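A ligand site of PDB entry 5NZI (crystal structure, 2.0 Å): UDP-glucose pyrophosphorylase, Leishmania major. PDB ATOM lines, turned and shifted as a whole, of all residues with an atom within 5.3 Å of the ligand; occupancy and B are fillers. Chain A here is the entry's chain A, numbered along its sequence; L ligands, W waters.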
ATOM      1  N   LEU A  81       4.395  15.984  29.537  1.00  0.00           N
ATOM      2  CA  LEU A  81       4.258  17.414  29.704  1.00  0.00           C
ATOM      3  C   LEU A  81       2.874  17.702  30.248  1.00  0.00           C
ATOM      4  O   LEU A  81       1.887  17.149  29.773  1.00  0.00           O
ATOM      5  CB  LEU A  81       4.445  18.130  28.391  1.00  0.00           C
ATOM      6  CG  LEU A  81       5.772  17.857  27.719  1.00  0.00           C
ATOM      7  CD1 LEU A  81       5.688  18.521  26.365  1.00  0.00           C
ATOM      8  CD2 LEU A  81       6.957  18.466  28.568  1.00  0.00           C
ATOM      9  N   ASN A  82       2.808  18.585  31.220  1.00  0.00           N
ATOM     10  CA  ASN A  82       1.565  18.816  31.937  1.00  0.00           C
ATOM     11  C   ASN A  82       1.543  20.206  32.520  1.00  0.00           C
ATOM     12  O   ASN A  82       1.006  20.393  33.618  1.00  0.00           O
ATOM     13  CB  ASN A  82       1.388  17.822  33.108  1.00  0.00           C
ATOM     14  CG  ASN A  82      -0.024  17.832  33.658  1.00  0.00           C
ATOM     15  OD1 ASN A  82      -0.967  17.896  32.899  1.00  0.00           O
ATOM     16  ND2 ASN A  82      -0.180  17.727  34.956  1.00  0.00           N
ATOM     17  N   GLY A  83       2.158  21.181  31.846  1.00  0.00           N
ATOM     18  CA  GLY A  83       2.358  22.483  32.464  1.00  0.00           C
ATOM     19  C   GLY A  83       1.643  23.641  31.810  1.00  0.00           C
ATOM     20  O   GLY A  83       1.634  24.741  32.352  1.00  0.00           O
ATOM     21  N   GLY A  84       1.129  23.451  30.625  1.00  0.00           N
ATOM     22  CA  GLY A  84       0.461  24.503  29.934  1.00  0.00           C
ATOM     23  C   GLY A  84      -0.954  24.742  30.331  1.00  0.00           C
ATOM     24  O   GLY A  84      -1.488  24.074  31.129  1.00  0.00           O
ATOM     25  N   LEU A  85      -1.509  25.793  29.812  1.00  0.00           N
ATOM     26  CA  LEU A  85      -2.875  26.102  30.021  1.00  0.00           C
ATOM     27  C   LEU A  85      -3.579  26.205  28.698  1.00  0.00           C
ATOM     28  O   LEU A  85      -3.342  27.134  27.978  1.00  0.00           O
ATOM     29  CB  LEU A  85      -2.962  27.456  30.637  1.00  0.00           C
ATOM     30  CG  LEU A  85      -2.909  27.604  32.131  1.00  0.00           C
ATOM     31  CD1 LEU A  85      -3.633  28.867  32.497  1.00  0.00           C
ATOM     32  CD2 LEU A  85      -3.502  26.410  32.832  1.00  0.00           C
ATOM     33  N   LYS A  95      -5.275  20.598  31.358  1.00  0.00           N
ATOM     34  CA  LYS A  95      -6.050  19.983  30.306  1.00  0.00           C
ATOM     35  C   LYS A  95      -6.209  18.490  30.556  1.00  0.00           C
ATOM     36  O   LYS A  95      -7.280  17.932  30.284  1.00  0.00           O
ATOM     37  CB  LYS A  95      -5.380  20.227  28.966  1.00  0.00           C
ATOM     38  CG  LYS A  95      -6.225  19.679  27.804  1.00  0.00           C
ATOM     39  CD  LYS A  95      -5.535  19.835  26.489  1.00  0.00           C
ATOM     40  CE  LYS A  95      -5.582  21.261  26.020  1.00  0.00           C
ATOM     41  NZ  LYS A  95      -5.026  21.350  24.651  1.00  0.00           N
ATOM     42  N   MET A 130       5.760  16.989  34.064  1.00  0.00           N
ATOM     43  CA  MET A 130       6.224  18.356  34.213  1.00  0.00           C
ATOM     44  C   MET A 130       4.992  19.215  34.435  1.00  0.00           C
ATOM     45  O   MET A 130       4.163  19.365  33.510  1.00  0.00           O
ATOM     46  CB  MET A 130       7.040  18.815  33.020  1.00  0.00           C
ATOM     47  CG  MET A 130       7.646  20.182  33.271  1.00  0.00           C
ATOM     48  SD  MET A 130       8.702  20.712  31.953  1.00  0.00           S
ATOM     49  CE  MET A 130       7.577  21.436  30.738  1.00  0.00           C
ATOM     50  N   GLN A 162       8.102  23.231  36.449  1.00  0.00           N
ATOM     51  CA  GLN A 162       8.797  24.017  35.468  1.00  0.00           C
ATOM     52  C   GLN A 162       9.014  25.431  35.995  1.00  0.00           C
ATOM     53  O   GLN A 162       8.412  25.848  36.981  1.00  0.00           O
ATOM     54  CB  GLN A 162       8.044  23.961  34.148  1.00  0.00           C
ATOM     55  CG  GLN A 162       7.156  25.064  33.821  1.00  0.00           C
ATOM     56  CD  GLN A 162       6.592  24.842  32.425  1.00  0.00           C
ATOM     57  OE1 GLN A 162       5.509  24.247  32.271  1.00  0.00           O
ATOM     58  NE2 GLN A 162       7.353  25.286  31.393  1.00  0.00           N
ATOM     59  N   PRO A 188       5.249  30.552  32.600  1.00  0.00           N
ATOM     60  CA  PRO A 188       6.144  29.439  32.232  1.00  0.00           C
ATOM     61  C   PRO A 188       6.664  29.642  30.818  1.00  0.00           C
ATOM     62  O   PRO A 188       5.937  30.156  29.952  1.00  0.00           O
ATOM     63  CB  PRO A 188       5.230  28.207  32.350  1.00  0.00           C
ATOM     64  CG  PRO A 188       3.840  28.752  32.084  1.00  0.00           C
ATOM     65  CD  PRO A 188       3.854  30.098  32.774  1.00  0.00           C
ATOM     66  N   PRO A 189       7.920  29.273  30.550  1.00  0.00           N
ATOM     67  CA  PRO A 189       8.544  29.681  29.280  1.00  0.00           C
ATOM     68  C   PRO A 189       8.439  28.648  28.155  1.00  0.00           C
ATOM     69  O   PRO A 189       9.379  28.425  27.378  1.00  0.00           O
ATOM     70  CB  PRO A 189      10.010  29.943  29.667  1.00  0.00           C
ATOM     71  CG  PRO A 189      10.257  28.988  30.799  1.00  0.00           C
ATOM     72  CD  PRO A 189       8.910  28.798  31.530  1.00  0.00           C
ATOM     73  N   GLY A 190       7.263  28.055  28.041  1.00  0.00           N
ATOM     74  CA  GLY A 190       7.011  27.029  27.059  1.00  0.00           C
ATOM     75  C   GLY A 190       7.615  25.711  27.497  1.00  0.00           C
ATOM     76  O   GLY A 190       8.358  25.626  28.483  1.00  0.00           O
ATOM     77  N   HIS A 191       7.323  24.665  26.696  1.00  0.00           N
ATOM     78  CA  HIS A 191       7.800  23.352  27.097  1.00  0.00           C
ATOM     79  C   HIS A 191       9.275  23.105  26.743  1.00  0.00           C
ATOM     80  O   HIS A 191       9.837  22.106  27.206  1.00  0.00           O
ATOM     81  CB  HIS A 191       6.900  22.241  26.523  1.00  0.00           C
ATOM     82  CG  HIS A 191       6.531  22.412  25.085  1.00  0.00           C
ATOM     83  ND1 HIS A 191       7.455  22.302  24.058  1.00  0.00           N
ATOM     84  CD2 HIS A 191       5.320  22.630  24.490  1.00  0.00           C
ATOM     85  CE1 HIS A 191       6.827  22.481  22.903  1.00  0.00           C
ATOM     86  NE2 HIS A 191       5.540  22.662  23.135  1.00  0.00           N
ATOM     87  N   ASN A 219       3.487  14.994  24.713  1.00  0.00           N
ATOM     88  CA  ASN A 219       2.414  15.887  25.147  1.00  0.00           C
ATOM     89  C   ASN A 219       1.441  15.184  26.069  1.00  0.00           C
ATOM     90  O   ASN A 219       1.061  14.031  25.849  1.00  0.00           O
ATOM     91  CB  ASN A 219       1.628  16.427  23.945  1.00  0.00           C
ATOM     92  CG  ASN A 219       2.419  17.457  23.172  1.00  0.00           C
ATOM     93  OD1 ASN A 219       3.465  17.943  23.680  1.00  0.00           O
ATOM     94  ND2 ASN A 219       2.001  17.747  21.930  1.00  0.00           N
ATOM     95  N   GLY A 220       0.999  15.911  27.095  1.00  0.00           N
ATOM     96  CA  GLY A 220       0.000  15.381  27.986  1.00  0.00           C
ATOM     97  C   GLY A 220      -1.282  15.006  27.260  1.00  0.00           C
ATOM     98  O   GLY A 220      -1.930  14.031  27.621  1.00  0.00           O
ATOM     99  N   ASP A 221      -1.643  15.756  26.216  1.00  0.00           N
ATOM    100  CA  ASP A 221      -2.873  15.518  25.463  1.00  0.00           C
ATOM    101  C   ASP A 221      -2.768  14.379  24.458  1.00  0.00           C
ATOM    102  O   ASP A 221      -3.801  13.990  23.899  1.00  0.00           O
ATOM    103  CB  ASP A 221      -3.307  16.795  24.729  1.00  0.00           C
ATOM    104  CG  ASP A 221      -2.292  17.268  23.681  1.00  0.00           C
ATOM    105  OD1 ASP A 221      -1.339  17.981  24.067  1.00  0.00           O
ATOM    106  OD2 ASP A 221      -2.473  16.981  22.478  1.00  0.00           O
ATOM    107  N   LYS A 255      -2.312  23.302  14.311  1.00  0.00           N
ATOM    108  CA  LYS A 255      -1.752  23.911  15.517  1.00  0.00           C
ATOM    109  C   LYS A 255      -0.542  23.089  15.971  1.00  0.00           C
ATOM    110  O   LYS A 255      -0.708  21.970  16.488  1.00  0.00           O
ATOM    111  CB  LYS A 255      -2.776  24.020  16.653  1.00  0.00           C
ATOM    112  CG  LYS A 255      -4.074  24.701  16.211  1.00  0.00           C
ATOM    113  CD  LYS A 255      -4.998  24.852  17.386  1.00  0.00           C
ATOM    114  CE  LYS A 255      -5.016  26.287  17.843  1.00  0.00           C
ATOM    115  NZ  LYS A 255      -5.838  27.012  16.814  1.00  0.00           N
ATOM    116  N   GLY A 256       0.652  23.642  15.813  1.00  0.00           N
ATOM    117  CA  GLY A 256       1.877  22.892  16.134  1.00  0.00           C
ATOM    118  C   GLY A 256       3.036  23.394  15.282  1.00  0.00           C
ATOM    119  O   GLY A 256       3.117  24.587  14.953  1.00  0.00           O
ATOM    120  N   GLY A 257       3.960  22.480  14.979  1.00  0.00           N
ATOM    121  CA  GLY A 257       5.087  22.815  14.140  1.00  0.00           C
ATOM    122  C   GLY A 257       5.365  21.676  13.191  1.00  0.00           C
ATOM    123  O   GLY A 257       4.899  20.552  13.359  1.00  0.00           O
ATOM    124  N   LEU A 282      12.844  22.690  13.778  1.00  0.00           N
ATOM    125  CA  LEU A 282      11.413  22.774  14.012  1.00  0.00           C
ATOM    126  C   LEU A 282      10.955  24.198  13.748  1.00  0.00           C
ATOM    127  O   LEU A 282      11.628  25.145  14.125  1.00  0.00           O
ATOM    128  CB  LEU A 282      11.082  22.358  15.443  1.00  0.00           C
ATOM    129  CG  LEU A 282       9.621  22.464  15.903  1.00  0.00           C
ATOM    130  CD1 LEU A 282       8.714  21.456  15.161  1.00  0.00           C
ATOM    131  CD2 LEU A 282       9.581  22.219  17.402  1.00  0.00           C
ATOM    132  N   GLU A 284       7.528  26.060  14.674  1.00  0.00           N
ATOM    133  CA  GLU A 284       6.218  26.227  15.306  1.00  0.00           C
ATOM    134  C   GLU A 284       5.388  27.219  14.521  1.00  0.00           C
ATOM    135  O   GLU A 284       5.912  28.085  13.831  1.00  0.00           O
ATOM    136  CB  GLU A 284       6.406  26.756  16.748  1.00  0.00           C
ATOM    137  CG  GLU A 284       7.054  25.785  17.678  1.00  0.00           C
ATOM    138  CD  GLU A 284       6.255  24.481  17.775  1.00  0.00           C
ATOM    139  OE1 GLU A 284       6.450  23.592  16.912  1.00  0.00           O
ATOM    140  OE2 GLU A 284       5.407  24.338  18.678  1.00  0.00           O
ATOM    141  N   PHE A 305       4.812  16.648  10.204  1.00  0.00           N
ATOM    142  CA  PHE A 305       4.315  17.360  11.366  1.00  0.00           C
ATOM    143  C   PHE A 305       4.964  16.776  12.621  1.00  0.00           C
ATOM    144  O   PHE A 305       4.957  15.559  12.803  1.00  0.00           O
ATOM    145  CB  PHE A 305       2.792  17.237  11.427  1.00  0.00           C
ATOM    146  CG  PHE A 305       2.098  18.326  12.184  1.00  0.00           C
ATOM    147  CD1 PHE A 305       2.015  19.619  11.675  1.00  0.00           C
ATOM    148  CD2 PHE A 305       1.519  18.071  13.439  1.00  0.00           C
ATOM    149  CE1 PHE A 305       1.355  20.654  12.389  1.00  0.00           C
ATOM    150  CE2 PHE A 305       0.898  19.088  14.168  1.00  0.00           C
ATOM    151  CZ  PHE A 305       0.795  20.371  13.631  1.00  0.00           C
ATOM    152  N   ASN A 306       5.529  17.644  13.461  1.00  0.00           N
ATOM    153  CA  ASN A 306       6.052  17.193  14.752  1.00  0.00           C
ATOM    154  C   ASN A 306       4.947  16.629  15.646  1.00  0.00           C
ATOM    155  O   ASN A 306       3.911  17.277  15.840  1.00  0.00           O
ATOM    156  CB  ASN A 306       6.795  18.341  15.463  1.00  0.00           C
ATOM    157  CG  ASN A 306       7.301  17.927  16.812  1.00  0.00           C
ATOM    158  OD1 ASN A 306       7.528  16.748  17.049  1.00  0.00           O
ATOM    159  ND2 ASN A 306       7.447  18.899  17.722  1.00  0.00           N
ATOM    160  N   THR A 307       5.149  15.408  16.164  1.00  0.00           N
ATOM    161  CA  THR A 307       4.218  14.803  17.120  1.00  0.00           C
ATOM    162  C   THR A 307       4.473  15.277  18.545  1.00  0.00           C
ATOM    163  O   THR A 307       3.567  15.160  19.398  1.00  0.00           O
ATOM    164  CB  THR A 307       4.321  13.289  17.108  1.00  0.00           C
ATOM    165  OG1 THR A 307       5.619  12.865  17.515  1.00  0.00           O
ATOM    166  CG2 THR A 307       3.921  12.650  15.679  1.00  0.00           C
ATOM    167  N   ASN A 308       5.675  15.815  18.792  1.00  0.00           N
ATOM    168  CA  ASN A 308       6.253  16.071  20.119  1.00  0.00           C
ATOM    169  C   ASN A 308       6.467  14.781  20.889  1.00  0.00           C
ATOM    170  O   ASN A 308       6.622  14.818  22.111  1.00  0.00           O
ATOM    171  CB  ASN A 308       5.414  17.075  20.932  1.00  0.00           C
ATOM    172  CG  ASN A 308       6.231  18.268  21.454  1.00  0.00           C
ATOM    173  OD1 ASN A 308       7.269  18.594  20.912  1.00  0.00           O
ATOM    174  ND2 ASN A 308       5.747  18.927  22.491  1.00  0.00           N
ATOM    175  N   ALA A 355      10.336  25.761  22.446  1.00  0.00           N
ATOM    176  CA  ALA A 355       9.620  24.512  22.222  1.00  0.00           C
ATOM    177  C   ALA A 355      10.581  23.347  22.337  1.00  0.00           C
ATOM    178  O   ALA A 355      11.674  23.392  21.758  1.00  0.00           O
ATOM    179  CB  ALA A 355       8.988  24.535  20.826  1.00  0.00           C
ATOM    180  N   PHE A 376      -0.066   9.362  17.505  1.00  0.00           N
ATOM    181  CA  PHE A 376      -0.345  10.792  17.570  1.00  0.00           C
ATOM    182  C   PHE A 376      -1.866  10.982  17.548  1.00  0.00           C
ATOM    183  O   PHE A 376      -2.503  10.864  16.488  1.00  0.00           O
ATOM    184  CB  PHE A 376       0.345  11.493  16.412  1.00  0.00           C
ATOM    185  CG  PHE A 376       0.236  12.992  16.441  1.00  0.00           C
ATOM    186  CD1 PHE A 376       0.716  13.709  17.525  1.00  0.00           C
ATOM    187  CD2 PHE A 376      -0.301  13.697  15.361  1.00  0.00           C
ATOM    188  CE1 PHE A 376       0.638  15.090  17.562  1.00  0.00           C
ATOM    189  CE2 PHE A 376      -0.409  15.097  15.412  1.00  0.00           C
ATOM    190  CZ  PHE A 376       0.101  15.784  16.535  1.00  0.00           C
ATOM    191  N   PRO A 378      -3.708  14.047  18.974  1.00  0.00           N
ATOM    192  CA  PRO A 378      -3.561  15.294  19.735  1.00  0.00           C
ATOM    193  C   PRO A 378      -4.928  15.860  20.041  1.00  0.00           C
ATOM    194  O   PRO A 378      -5.916  15.515  19.411  1.00  0.00           O
ATOM    195  CB  PRO A 378      -2.807  16.220  18.789  1.00  0.00           C
ATOM    196  CG  PRO A 378      -3.313  15.705  17.351  1.00  0.00           C
ATOM    197  CD  PRO A 378      -3.364  14.194  17.552  1.00  0.00           C
ATOM    198  N   LYS A 380      -5.806  19.746  20.535  1.00  0.00           N
ATOM    199  CA  LYS A 380      -5.569  21.176  20.717  1.00  0.00           C
ATOM    200  C   LYS A 380      -6.856  21.990  20.899  1.00  0.00           C
ATOM    201  O   LYS A 380      -6.792  23.098  21.448  1.00  0.00           O
ATOM    202  CB  LYS A 380      -4.805  21.755  19.542  1.00  0.00           C
ATOM    203  CG  LYS A 380      -3.394  21.207  19.391  1.00  0.00           C
ATOM    204  CD  LYS A 380      -2.785  20.790  20.753  1.00  0.00           C
ATOM    205  CE  LYS A 380      -1.441  20.157  20.467  1.00  0.00           C
ATOM    206  NZ  LYS A 380      -0.939  19.141  21.447  1.00  0.00           N
HETATM  207  N1  LIG L   1       3.170  22.673  28.057  1.00  0.00           N
HETATM  208  C1  LIG L   1       3.898  22.772  29.216  1.00  0.00           C
HETATM  209  N2  LIG L   1       4.424  23.921  29.504  1.00  0.00           N
HETATM  210  C2  LIG L   1       4.297  24.959  28.770  1.00  0.00           C
HETATM  211  C3  LIG L   1       3.540  24.849  27.604  1.00  0.00           C
HETATM  212  C4  LIG L   1       3.014  23.709  27.287  1.00  0.00           C
HETATM  213  O1  LIG L   1       4.116  21.893  29.930  1.00  0.00           O
HETATM  214  O2  LIG L   1       4.800  25.874  29.144  1.00  0.00           O
HETATM  215  C5  LIG L   1       2.610  21.409  27.721  1.00  0.00           C
HETATM  216  C6  LIG L   1       1.142  21.506  27.385  1.00  0.00           C
HETATM  217  O3  LIG L   1       0.495  21.375  28.458  1.00  0.00           O
HETATM  218  C7  LIG L   1       1.046  20.297  26.463  1.00  0.00           C
HETATM  219  C8  LIG L   1       2.350  20.304  25.831  1.00  0.00           C
HETATM  220  O4  LIG L   1       3.195  21.016  26.609  1.00  0.00           O
HETATM  221  O5  LIG L   1       0.990  19.151  27.090  1.00  0.00           O
HETATM  222  C9  LIG L   1       2.273  20.960  24.461  1.00  0.00           C
HETATM  223  O6  LIG L   1       1.611  22.111  24.442  1.00  0.00           O
HETATM  224  P1  LIG L   1       0.532  22.473  23.282  1.00  0.00           P
HETATM  225  O7  LIG L   1       0.289  23.830  23.541  1.00  0.00           O
HETATM  226  O8  LIG L   1      -0.437  21.564  23.562  1.00  0.00           O
HETATM  227  O9  LIG L   1       1.128  22.345  21.923  1.00  0.00           O
HETATM  228  P2  LIG L   1       2.009  23.179  21.113  1.00  0.00           P
HETATM  229  O10 LIG L   1       3.037  23.654  21.928  1.00  0.00           O
HETATM  230  O11 LIG L   1       1.449  24.134  20.314  1.00  0.00           O
HETATM  231  O12 LIG L   1       2.800  22.240  20.058  1.00  0.00           O
HETATM  232  C10 LIG L   1       3.482  21.121  20.310  1.00  0.00           C
HETATM  233  C11 LIG L   1       4.814  21.159  19.653  1.00  0.00           C
HETATM  234  C12 LIG L   1       4.582  21.225  18.146  1.00  0.00           C
HETATM  235  C13 LIG L   1       3.866  19.945  17.771  1.00  0.00           C
HETATM  236  C14 LIG L   1       2.562  19.910  18.570  1.00  0.00           C
HETATM  237  C15 LIG L   1       1.827  18.658  18.208  1.00  0.00           C
HETATM  238  O13 LIG L   1       5.449  22.222  19.936  1.00  0.00           O
HETATM  239  O14 LIG L   1       5.730  21.265  17.488  1.00  0.00           O
HETATM  240  O15 LIG L   1       3.501  19.976  16.517  1.00  0.00           O
HETATM  241  O16 LIG L   1       2.866  19.970  19.873  1.00  0.00           O
HETATM  242  O17 LIG L   1       0.779  18.412  18.911  1.00  0.00           O
HETATM  243  O   HOH W   1       5.242  25.804  21.221  1.00  0.00           O
HETATM  244  O   HOH W   2       8.367  21.096  20.406  1.00  0.00           O
HETATM  245  O   HOH W   3       2.875  25.866  24.203  1.00  0.00           O
HETATM  246  O   HOH W   4      -2.288  20.461  25.395  1.00  0.00           O
HETATM  247  O   HOH W   5      -1.472  18.568  28.037  1.00  0.00           O
HETATM  248  O   HOH W   6      -2.262  22.688  27.762  1.00  0.00           O
HETATM  249  O   HOH W   7       2.720  25.475  18.225  1.00  0.00           O
HETATM  250  O   HOH W   8      -0.118  24.958  25.936  1.00  0.00           O
HETATM  251  O   HOH W   9      -0.275  16.443  20.814  1.00  0.00           O
HETATM  252  O   HOH W  10      -1.205  19.256  16.878  1.00  0.00           O
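The side-chain carboxylate of Glu 284 sits at hydrogen-bond distance from an oxygen (O13) of the ligand, at 2.5 Å.
The backbone carbonyl oxygen of Asn 306 lies within hydrogen-bond range of an oxygen (O15) of the ligand (2.8 Å).
An oxygen (O14) of the ligand sits at hydrogen-bond distance from the side-chain amide nitrogen (ND2) of Asn 306.
The backbone NH of Gly 83 is in hydrogen-bond range of an oxygen (O1) of the ligand (2.8 Å).
A ring nitrogen (NE2) of His 191 is in hydrogen-bond range of an oxygen (O10) of the ligand (3.0 Å).
An oxygen (O15) of the ligand sits at hydrogen-bond distance from the backbone NH (N) of Gly 257 (3.0 Å).
The side-chain amide oxygen (OE1) of Gln 162 is in hydrogen-bond range of a nitrogen (N2) of the ligand.
The backbone NH of Gly 84 is in hydrogen-bond range of an oxygen (O3) of the ligand.
NZ of Lys 380 lies within salt-bridge range of O8 of the ligand (3.3 Å).
The side-chain amide nitrogen (ND2) of Asn 219 is in hydrogen-bond range of an oxygen (O16) of the ligand, 3.1 Å away.
The backbone NH (N) of Gly 220 is in hydrogen-bond range of an oxygen (O5) of the ligand (3.2 Å).
O2 of the ligand lies close to N of Gly 190 (3.5 Å).
The backbone carbonyl oxygen (O) of Leu 81 lies within hydrogen-bond range of an oxygen (O5) of the ligand, 3.5 Å away.
Water W5 bridges an oxygen (O5) of the ligand (2.7 Å) and the backbone NH (N) of Asp 221 (3.4 Å).
Water W7 lies within hydrogen-bond range of O11 of the ligand (2.8 Å), OE2 of Glu 284 (3.0 Å) and O of Gly 256 (3.4 Å).
Water W9 lies within hydrogen-bond range of OD2 of Asp 221 (2.8 Å), NZ of Lys 380 (2.8 Å), ND2 of Asn 219 (2.9 Å) and O17 of the ligand (2.9 Å).
Water W10 lies within hydrogen-bond range of the backbone carbonyl oxygen (O) of Lys 255 (2.8 Å) and an oxygen (O17) of the ligand (3.0 Å).
Water W1 bridges the side-chain carboxylate (OE2) of Glu 284 and an oxygen (O10) of the ligand.
Water W2 lies within hydrogen-bond range of OD1 of Asn 308 (2.8 Å) and O13 of the ligand (3.2 Å).
The side-chain carboxylate (OE1) of Glu 284 sits close to the backbone NH (N) of Gly 257, at 3.3 Å.
N of Asn 306 sits at hydrogen-bond distance from O of Gly 257 (3.0 Å).
The backbone NH (N) of Asn 308 sits at hydrogen-bond distance from the side-chain amide oxygen (OD1) of Asn 306, 2.7 Å away.
O of Gly 190 lies within hydrogen-bond range of NE2 of Gln 162 (3.1 Å).
The side-chain amino group (NZ) of Lys 380 sits close to the side-chain amide nitrogen (ND2) of Asn 219, at 3.3 Å.
The side-chain carboxylate of Asp 221 lies within salt-bridge range of the side-chain amino group of Lys 380.
The side-chain amide oxygen of Asn 219 is in hydrogen-bond range of the side-chain amide nitrogen of Asn 308, at 2.8 Å.
O of Met 130 lies within hydrogen-bond range of N of Asn 82, 2.8 Å away.
N of Asn 82 touches O1 of the ligand, 3.8 Å away.
Met 130 touches the ligand.
Pro 188 touches the ligand (CB to O2, 3.99 Å).
OD1 of Asp 221 touches O8 of the ligand (3.7 Å).
CA of Gly 256 touches O15 of the ligand, at 3.4 Å.
Leu 282 touches the ligand.
CE2 of Phe 305 touches O15 of the ligand (3.6 Å).
Asn 308 touches the ligand.
CE1 of Phe 376 touches O17 of the ligand, at 3.6 Å.
Hydrophobic or aromatic side chains that line the ligand: Leu 81, Met 130, Pro 188, His 191, Leu 282, Phe 305 and Phe 376.
The nearest printed residue that does not touch the ligand is Thr 307 (4.1 Å).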
